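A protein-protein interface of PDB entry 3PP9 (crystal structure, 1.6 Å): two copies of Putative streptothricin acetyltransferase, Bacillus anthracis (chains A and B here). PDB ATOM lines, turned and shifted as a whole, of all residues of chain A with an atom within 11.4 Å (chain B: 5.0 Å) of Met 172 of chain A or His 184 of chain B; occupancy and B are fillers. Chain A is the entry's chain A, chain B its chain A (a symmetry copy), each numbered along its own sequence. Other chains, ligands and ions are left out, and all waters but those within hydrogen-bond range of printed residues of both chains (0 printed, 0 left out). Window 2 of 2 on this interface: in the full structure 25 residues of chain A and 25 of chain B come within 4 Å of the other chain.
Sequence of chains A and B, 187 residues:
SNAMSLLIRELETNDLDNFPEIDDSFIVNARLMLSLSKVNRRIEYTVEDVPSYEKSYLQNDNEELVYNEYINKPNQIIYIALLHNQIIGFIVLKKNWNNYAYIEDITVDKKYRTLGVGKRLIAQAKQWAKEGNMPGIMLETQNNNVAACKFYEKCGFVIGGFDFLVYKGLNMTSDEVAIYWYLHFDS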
ATOM      1  N   PHE A 164       8.726 -13.782   1.730  1.00  0.00           N
ATOM      2  CA  PHE A 164      10.116 -13.560   1.330  1.00  0.00           C
ATOM      3  C   PHE A 164      10.322 -12.798   0.033  1.00  0.00           C
ATOM      4  O   PHE A 164      11.460 -12.381  -0.243  1.00  0.00           O
ATOM      5  CB  PHE A 164      10.844 -14.900   1.090  1.00  0.00           C
ATOM      6  CG  PHE A 164      10.884 -15.810   2.276  1.00  0.00           C
ATOM      7  CD1 PHE A 164      11.549 -15.437   3.427  1.00  0.00           C
ATOM      8  CD2 PHE A 164      10.364 -17.090   2.194  1.00  0.00           C
ATOM      9  CE1 PHE A 164      11.620 -16.297   4.530  1.00  0.00           C
ATOM     10  CE2 PHE A 164      10.440 -17.962   3.284  1.00  0.00           C
ATOM     11  CZ  PHE A 164      11.078 -17.549   4.456  1.00  0.00           C
ATOM     12  N   LEU A 165       9.277 -12.606  -0.763  1.00  0.00           N
ATOM     13  CA  LEU A 165       9.448 -11.955  -2.047  1.00  0.00           C
ATOM     14  C   LEU A 165       8.739 -10.632  -2.237  1.00  0.00           C
ATOM     15  O   LEU A 165       9.104  -9.883  -3.147  1.00  0.00           O
ATOM     16  CB  LEU A 165       9.002 -12.914  -3.162  1.00  0.00           C
ATOM     17  CG  LEU A 165       9.790 -14.230  -3.280  1.00  0.00           C
ATOM     18  CD1 LEU A 165       9.265 -15.105  -4.419  1.00  0.00           C
ATOM     19  CD2 LEU A 165      11.266 -13.974  -3.495  1.00  0.00           C
ATOM     20  N   VAL A 166       7.771 -10.314  -1.392  1.00  0.00           N
ATOM     21  CA  VAL A 166       7.006  -9.075  -1.618  1.00  0.00           C
ATOM     22  C   VAL A 166       7.924  -7.832  -1.687  1.00  0.00           C
ATOM     23  O   VAL A 166       7.782  -6.970  -2.573  1.00  0.00           O
ATOM     24  CB  VAL A 166       5.835  -8.934  -0.661  1.00  0.00           C
ATOM     25  CG1 VAL A 166       6.289  -8.694   0.786  1.00  0.00           C
ATOM     26  CG2 VAL A 166       4.876  -7.818  -1.166  1.00  0.00           C
ATOM     27  N   TYR A 167       8.927  -7.785  -0.817  1.00  0.00           N
ATOM     28  CA  TYR A 167       9.851  -6.630  -0.824  1.00  0.00           C
ATOM     29  C   TYR A 167      10.812  -6.523  -2.009  1.00  0.00           C
ATOM     30  O   TYR A 167      11.375  -5.434  -2.255  1.00  0.00           O
ATOM     31  CB  TYR A 167      10.606  -6.506   0.502  1.00  0.00           C
ATOM     32  CG  TYR A 167       9.750  -5.955   1.607  1.00  0.00           C
ATOM     33  CD1 TYR A 167       9.480  -4.594   1.666  1.00  0.00           C
ATOM     34  CD2 TYR A 167       9.250  -6.759   2.612  1.00  0.00           C
ATOM     35  CE1 TYR A 167       8.699  -4.063   2.659  1.00  0.00           C
ATOM     36  CE2 TYR A 167       8.460  -6.226   3.631  1.00  0.00           C
ATOM     37  CZ  TYR A 167       8.187  -4.880   3.642  1.00  0.00           C
ATOM     38  OH  TYR A 167       7.411  -4.330   4.643  1.00  0.00           O
ATOM     39  N   LYS A 168      10.996  -7.621  -2.736  1.00  0.00           N
ATOM     40  CA  LYS A 168      11.853  -7.660  -3.912  1.00  0.00           C
ATOM     41  C   LYS A 168      11.395  -6.681  -4.981  1.00  0.00           C
ATOM     42  O   LYS A 168      12.188  -6.243  -5.806  1.00  0.00           O
ATOM     43  CB  LYS A 168      11.801  -9.052  -4.541  1.00  0.00           C
ATOM     44  CG  LYS A 168      12.373 -10.169  -3.691  1.00  0.00           C
ATOM     45  CD  LYS A 168      13.879 -10.024  -3.572  1.00  0.00           C
ATOM     46  CE  LYS A 168      14.485 -11.163  -2.776  1.00  0.00           C
ATOM     47  NZ  LYS A 168      15.962 -11.042  -2.769  1.00  0.00           N
ATOM     48  N   GLY A 169      10.107  -6.346  -4.972  1.00  0.00           N
ATOM     49  CA  GLY A 169       9.547  -5.443  -5.980  1.00  0.00           C
ATOM     50  C   GLY A 169      10.117  -4.047  -5.830  1.00  0.00           C
ATOM     51  O   GLY A 169      10.191  -3.296  -6.796  1.00  0.00           O
ATOM     52  N   LEU A 170      10.494  -3.690  -4.607  1.00  0.00           N
ATOM     53  CA  LEU A 170      11.106  -2.384  -4.360  1.00  0.00           C
ATOM     54  C   LEU A 170      12.612  -2.515  -4.576  1.00  0.00           C
ATOM     55  O   LEU A 170      13.204  -1.761  -5.364  1.00  0.00           O
ATOM     56  CB  LEU A 170      10.797  -1.886  -2.951  1.00  0.00           C
ATOM     57  CG  LEU A 170       9.317  -1.688  -2.595  1.00  0.00           C
ATOM     58  CD1 LEU A 170       9.189  -1.193  -1.166  1.00  0.00           C
ATOM     59  CD2 LEU A 170       8.626  -0.723  -3.544  1.00  0.00           C
ATOM     60  N   ASN A 171      13.228  -3.476  -3.882  1.00  0.00           N
ATOM     61  CA  ASN A 171      14.678  -3.718  -3.989  1.00  0.00           C
ATOM     62  C   ASN A 171      15.068  -5.202  -4.094  1.00  0.00           C
ATOM     63  O   ASN A 171      14.876  -5.965  -3.153  1.00  0.00           O
ATOM     64  CB  ASN A 171      15.434  -3.113  -2.791  1.00  0.00           C
ATOM     65  CG  ASN A 171      15.303  -1.596  -2.697  1.00  0.00           C
ATOM     66  OD1 ASN A 171      14.275  -1.021  -3.044  1.00  0.00           O
ATOM     67  ND2 ASN A 171      16.338  -0.949  -2.178  1.00  0.00           N
ATOM     68  N   MET A 172      15.641  -5.578  -5.233  1.00  0.00           N
ATOM     69  CA  MET A 172      16.108  -6.949  -5.503  1.00  0.00           C
ATOM     70  C   MET A 172      17.408  -7.352  -4.801  1.00  0.00           C
ATOM     71  O   MET A 172      17.748  -8.536  -4.747  1.00  0.00           O
ATOM     72  CB  MET A 172      16.343  -7.107  -7.008  1.00  0.00           C
ATOM     73  CG  MET A 172      15.094  -7.250  -7.826  1.00  0.00           C
ATOM     74  SD  MET A 172      14.404  -9.063  -7.620  1.00  0.00           S
ATOM     75  CE  MET A 172      15.805 -10.044  -8.559  1.00  0.00           C
ATOM     76  N   THR A 173      18.136  -6.380  -4.269  1.00  0.00           N
ATOM     77  CA  THR A 173      19.415  -6.664  -3.621  1.00  0.00           C
ATOM     78  C   THR A 173      19.293  -7.194  -2.208  1.00  0.00           C
ATOM     79  O   THR A 173      20.029  -8.101  -1.806  1.00  0.00           O
ATOM     80  CB  THR A 173      20.273  -5.402  -3.563  1.00  0.00           C
ATOM     81  OG1 THR A 173      19.575  -4.388  -2.828  1.00  0.00           O
ATOM     82  CG2 THR A 173      20.559  -4.909  -4.961  1.00  0.00           C
ATOM     83  N   SER A 174      18.391  -6.598  -1.447  1.00  0.00           N
ATOM     84  CA  SER A 174      18.193  -6.996  -0.074  1.00  0.00           C
ATOM     85  C   SER A 174      17.227  -8.182   0.064  1.00  0.00           C
ATOM     86  O   SER A 174      16.537  -8.586  -0.879  1.00  0.00           O
ATOM     87  CB  SER A 174      17.751  -5.800   0.758  1.00  0.00           C
ATOM     88  OG  SER A 174      18.728  -4.775   0.739  1.00  0.00           O
ATOM     89  N   ASP A 175      17.192  -8.718   1.273  1.00  0.00           N
ATOM     90  CA  ASP A 175      16.420  -9.883   1.591  1.00  0.00           C
ATOM     91  C   ASP A 175      15.463  -9.646   2.759  1.00  0.00           C
ATOM     92  O   ASP A 175      15.371 -10.484   3.650  1.00  0.00           O
ATOM     93  CB  ASP A 175      17.417 -11.013   1.904  1.00  0.00           C
ATOM     94  CG  ASP A 175      18.274 -11.399   0.684  1.00  0.00           C
ATOM     95  OD1 ASP A 175      17.712 -11.512  -0.434  1.00  0.00           O
ATOM     96  OD2 ASP A 175      19.483 -11.633   0.855  1.00  0.00           O
ATOM     97  N   GLU A 176      14.732  -8.533   2.692  1.00  0.00           N
ATOM     98  CA  GLU A 176      13.756  -8.129   3.699  1.00  0.00           C
ATOM     99  C   GLU A 176      12.581  -9.112   3.679  1.00  0.00           C
ATOM    100  O   GLU A 176      12.150  -9.502   2.594  1.00  0.00           O
ATOM    101  CB  GLU A 176      13.251  -6.730   3.336  1.00  0.00           C
ATOM    102  CG  GLU A 176      14.380  -5.728   3.155  1.00  0.00           C
ATOM    103  CD  GLU A 176      13.929  -4.359   2.672  1.00  0.00           C
ATOM    104  OE1 GLU A 176      12.751  -4.199   2.308  1.00  0.00           O
ATOM    105  OE2 GLU A 176      14.773  -3.440   2.651  1.00  0.00           O
ATOM    106  N   VAL A 177      12.066  -9.500   4.851  1.00  0.00           N
ATOM    107  CA  VAL A 177      10.941 -10.439   4.924  1.00  0.00           C
ATOM    108  C   VAL A 177       9.780  -9.782   5.653  1.00  0.00           C
ATOM    109  O   VAL A 177       9.968  -9.168   6.704  1.00  0.00           O
ATOM    110  CB  VAL A 177      11.335 -11.722   5.701  1.00  0.00           C
ATOM    111  CG1 VAL A 177      10.196 -12.742   5.741  1.00  0.00           C
ATOM    112  CG2 VAL A 177      12.614 -12.374   5.100  1.00  0.00           C
ATOM    113  N   TYR B 100       4.727  -4.376  -8.228  1.00  0.00           N
ATOM    114  CA  TYR B 100       4.335  -5.475  -9.084  1.00  0.00           C
ATOM    115  C   TYR B 100       2.910  -5.329  -9.582  1.00  0.00           C
ATOM    116  O   TYR B 100       2.074  -4.657  -8.973  1.00  0.00           O
ATOM    117  CB  TYR B 100       4.385  -6.814  -8.305  1.00  0.00           C
ATOM    118  CG  TYR B 100       5.710  -7.542  -8.278  1.00  0.00           C
ATOM    119  CD1 TYR B 100       6.889  -6.880  -7.994  1.00  0.00           C
ATOM    120  CD2 TYR B 100       5.767  -8.921  -8.472  1.00  0.00           C
ATOM    121  CE1 TYR B 100       8.094  -7.552  -7.980  1.00  0.00           C
ATOM    122  CE2 TYR B 100       6.990  -9.602  -8.437  1.00  0.00           C
ATOM    123  CZ  TYR B 100       8.140  -8.899  -8.189  1.00  0.00           C
ATOM    124  OH  TYR B 100       9.387  -9.501  -8.133  1.00  0.00           O
ATOM    125  N   PRO B 135       8.198  -4.654 -12.287  1.00  0.00           N
ATOM    126  CA  PRO B 135       9.196  -5.716 -12.344  1.00  0.00           C
ATOM    127  C   PRO B 135       8.713  -7.157 -12.246  1.00  0.00           C
ATOM    128  O   PRO B 135       9.541  -8.073 -12.313  1.00  0.00           O
ATOM    129  CB  PRO B 135      10.117  -5.365 -11.172  1.00  0.00           C
ATOM    130  CG  PRO B 135       9.198  -4.773 -10.163  1.00  0.00           C
ATOM    131  CD  PRO B 135       8.191  -3.978 -10.978  1.00  0.00           C
ATOM    132  N   GLY B 136       7.409  -7.375 -12.106  1.00  0.00           N
ATOM    133  CA  GLY B 136       6.874  -8.717 -12.021  1.00  0.00           C
ATOM    134  C   GLY B 136       5.380  -8.685 -11.810  1.00  0.00           C
ATOM    135  O   GLY B 136       4.760  -7.615 -11.863  1.00  0.00           O
ATOM    136  N   TYR B 182       4.550 -15.353  -7.071  1.00  0.00           N
ATOM    137  CA  TYR B 182       5.313 -14.315  -7.735  1.00  0.00           C
ATOM    138  C   TYR B 182       5.994 -14.753  -9.010  1.00  0.00           C
ATOM    139  O   TYR B 182       6.543 -15.841  -9.073  1.00  0.00           O
ATOM    140  CB  TYR B 182       6.445 -13.865  -6.778  1.00  0.00           C
ATOM    141  CG  TYR B 182       5.907 -13.239  -5.512  1.00  0.00           C
ATOM    142  CD1 TYR B 182       5.731 -11.870  -5.407  1.00  0.00           C
ATOM    143  CD2 TYR B 182       5.512 -14.027  -4.440  1.00  0.00           C
ATOM    144  CE1 TYR B 182       5.175 -11.302  -4.258  1.00  0.00           C
ATOM    145  CE2 TYR B 182       4.956 -13.458  -3.295  1.00  0.00           C
ATOM    146  CZ  TYR B 182       4.830 -12.099  -3.200  1.00  0.00           C
ATOM    147  OH  TYR B 182       4.238 -11.566  -2.068  1.00  0.00           O
ATOM    148  N   LEU B 183       5.978 -13.875 -10.004  1.00  0.00           N
ATOM    149  CA  LEU B 183       6.684 -14.111 -11.271  1.00  0.00           C
ATOM    150  C   LEU B 183       7.507 -12.857 -11.489  1.00  0.00           C
ATOM    151  O   LEU B 183       6.950 -11.807 -11.777  1.00  0.00           O
ATOM    152  CB  LEU B 183       5.746 -14.307 -12.446  1.00  0.00           C
ATOM    153  CG  LEU B 183       6.388 -14.570 -13.816  1.00  0.00           C
ATOM    154  CD1 LEU B 183       7.148 -15.860 -13.801  1.00  0.00           C
ATOM    155  CD2 LEU B 183       5.316 -14.635 -14.877  1.00  0.00           C
ATOM    156  N   HIS B 184       8.825 -12.972 -11.345  1.00  0.00           N
ATOM    157  CA  HIS B 184       9.737 -11.840 -11.539  1.00  0.00           C
ATOM    158  C   HIS B 184      10.289 -11.837 -12.952  1.00  0.00           C
ATOM    159  O   HIS B 184      10.633 -12.882 -13.485  1.00  0.00           O
ATOM    160  CB  HIS B 184      10.901 -11.889 -10.538  1.00  0.00           C
ATOM    161  CG  HIS B 184      11.875 -10.762 -10.693  1.00  0.00           C
ATOM    162  ND1 HIS B 184      13.130 -10.929 -11.242  1.00  0.00           N
ATOM    163  CD2 HIS B 184      11.760  -9.443 -10.411  1.00  0.00           C
ATOM    164  CE1 HIS B 184      13.755  -9.763 -11.267  1.00  0.00           C
ATOM    165  NE2 HIS B 184      12.943  -8.845 -10.774  1.00  0.00           N
ATOM    166  N   PHE B 185      10.371 -10.664 -13.564  1.00  0.00           N
ATOM    167  CA  PHE B 185      10.895 -10.587 -14.913  1.00  0.00           C
ATOM    168  C   PHE B 185      12.415 -10.432 -14.884  1.00  0.00           C
ATOM    169  O   PHE B 185      12.946  -9.673 -14.069  1.00  0.00           O
ATOM    170  CB  PHE B 185      10.272  -9.434 -15.681  1.00  0.00           C
ATOM    171  CG  PHE B 185       8.768  -9.386 -15.605  1.00  0.00           C
ATOM    172  CD1 PHE B 185       8.003 -10.529 -15.777  1.00  0.00           C
ATOM    173  CD2 PHE B 185       8.121  -8.175 -15.484  1.00  0.00           C
ATOM    174  CE1 PHE B 185       6.627 -10.459 -15.744  1.00  0.00           C
ATOM    175  CE2 PHE B 185       6.757  -8.103 -15.471  1.00  0.00           C
ATOM    176  CZ  PHE B 185       6.015  -9.232 -15.606  1.00  0.00           C
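The side-chain sulfur (SD) of Met 172 of chain A is in hydrogen-bond range of a ring nitrogen (NE2) of His 184 of chain B (3.5 Å).
The backbone carbonyl oxygen of Pro 135 of chain B is in hydrogen-bond range of the backbone NH of Phe 185 of chain B, at 3.0 Å.
Among the printed residues, pairs that only touch across the chains: Leu 165 of chain A with Tyr 182 of chain B, Val 166 of chain A with Tyr 182 of chain B, Gly 169 of chain A with Tyr 100 of chain B and Gly 169 of chain A with Pro 135 of chain B.
Of the printed residues of chain B, Met 172 of chain A touches His 184.
His 184 of chain B touches one residue of chain A.
Pro 135 of chain B touches just one residue of chain A: Gly 169 (3.8 Å).
Printed residues of chain B within 4 Å of Leu 165 of chain A: Tyr 182.
Of the printed residues of chain B, Gly 169 of chain A touches Tyr 100 and Pro 135.
Printed residues of chain A within 4 Å of Tyr 182 of chain B: Leu 165 (3.9 Å) and Val 166 (3.4 Å).
Of the printed residues of chain A, Tyr 100 of chain B touches Gly 169.
Printed residues of chain B within 4 Å of Val 166 of chain A: Tyr 182.
Thr 173 of chain A touches none of the printed residues of chain B.
Lys 168 of chain A touches none of the printed residues of chain B.
The nearest printed residue of chain A that does not touch His 184 of chain B is Lys 168 of chain A (5.6 Å).
The nearest printed residue of chain A that does not touch Tyr 100 of chain B is Lys 168 of chain A (4.4 Å).
Of the 14 printed residues of chain A, 4 touch a printed residue of chain B.
Of the 7 printed residues of chain B, 4 touch a printed residue of chain A.
Hydrophobic or aromatic side chains of chain B within 4 Å of the printed part of chain A: Tyr 100, Pro 135, Tyr 182 and His 184.
Along chain B the printed residues that touch a printed residue of chain A span positions 100 to 184.
Among the printed residues, 5 pairs touch across the chains.
No position is printed for both chains.
Of the 5 pairs that touch across the chains among the printed residues, none has its exchanged pair printed and touching as well.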
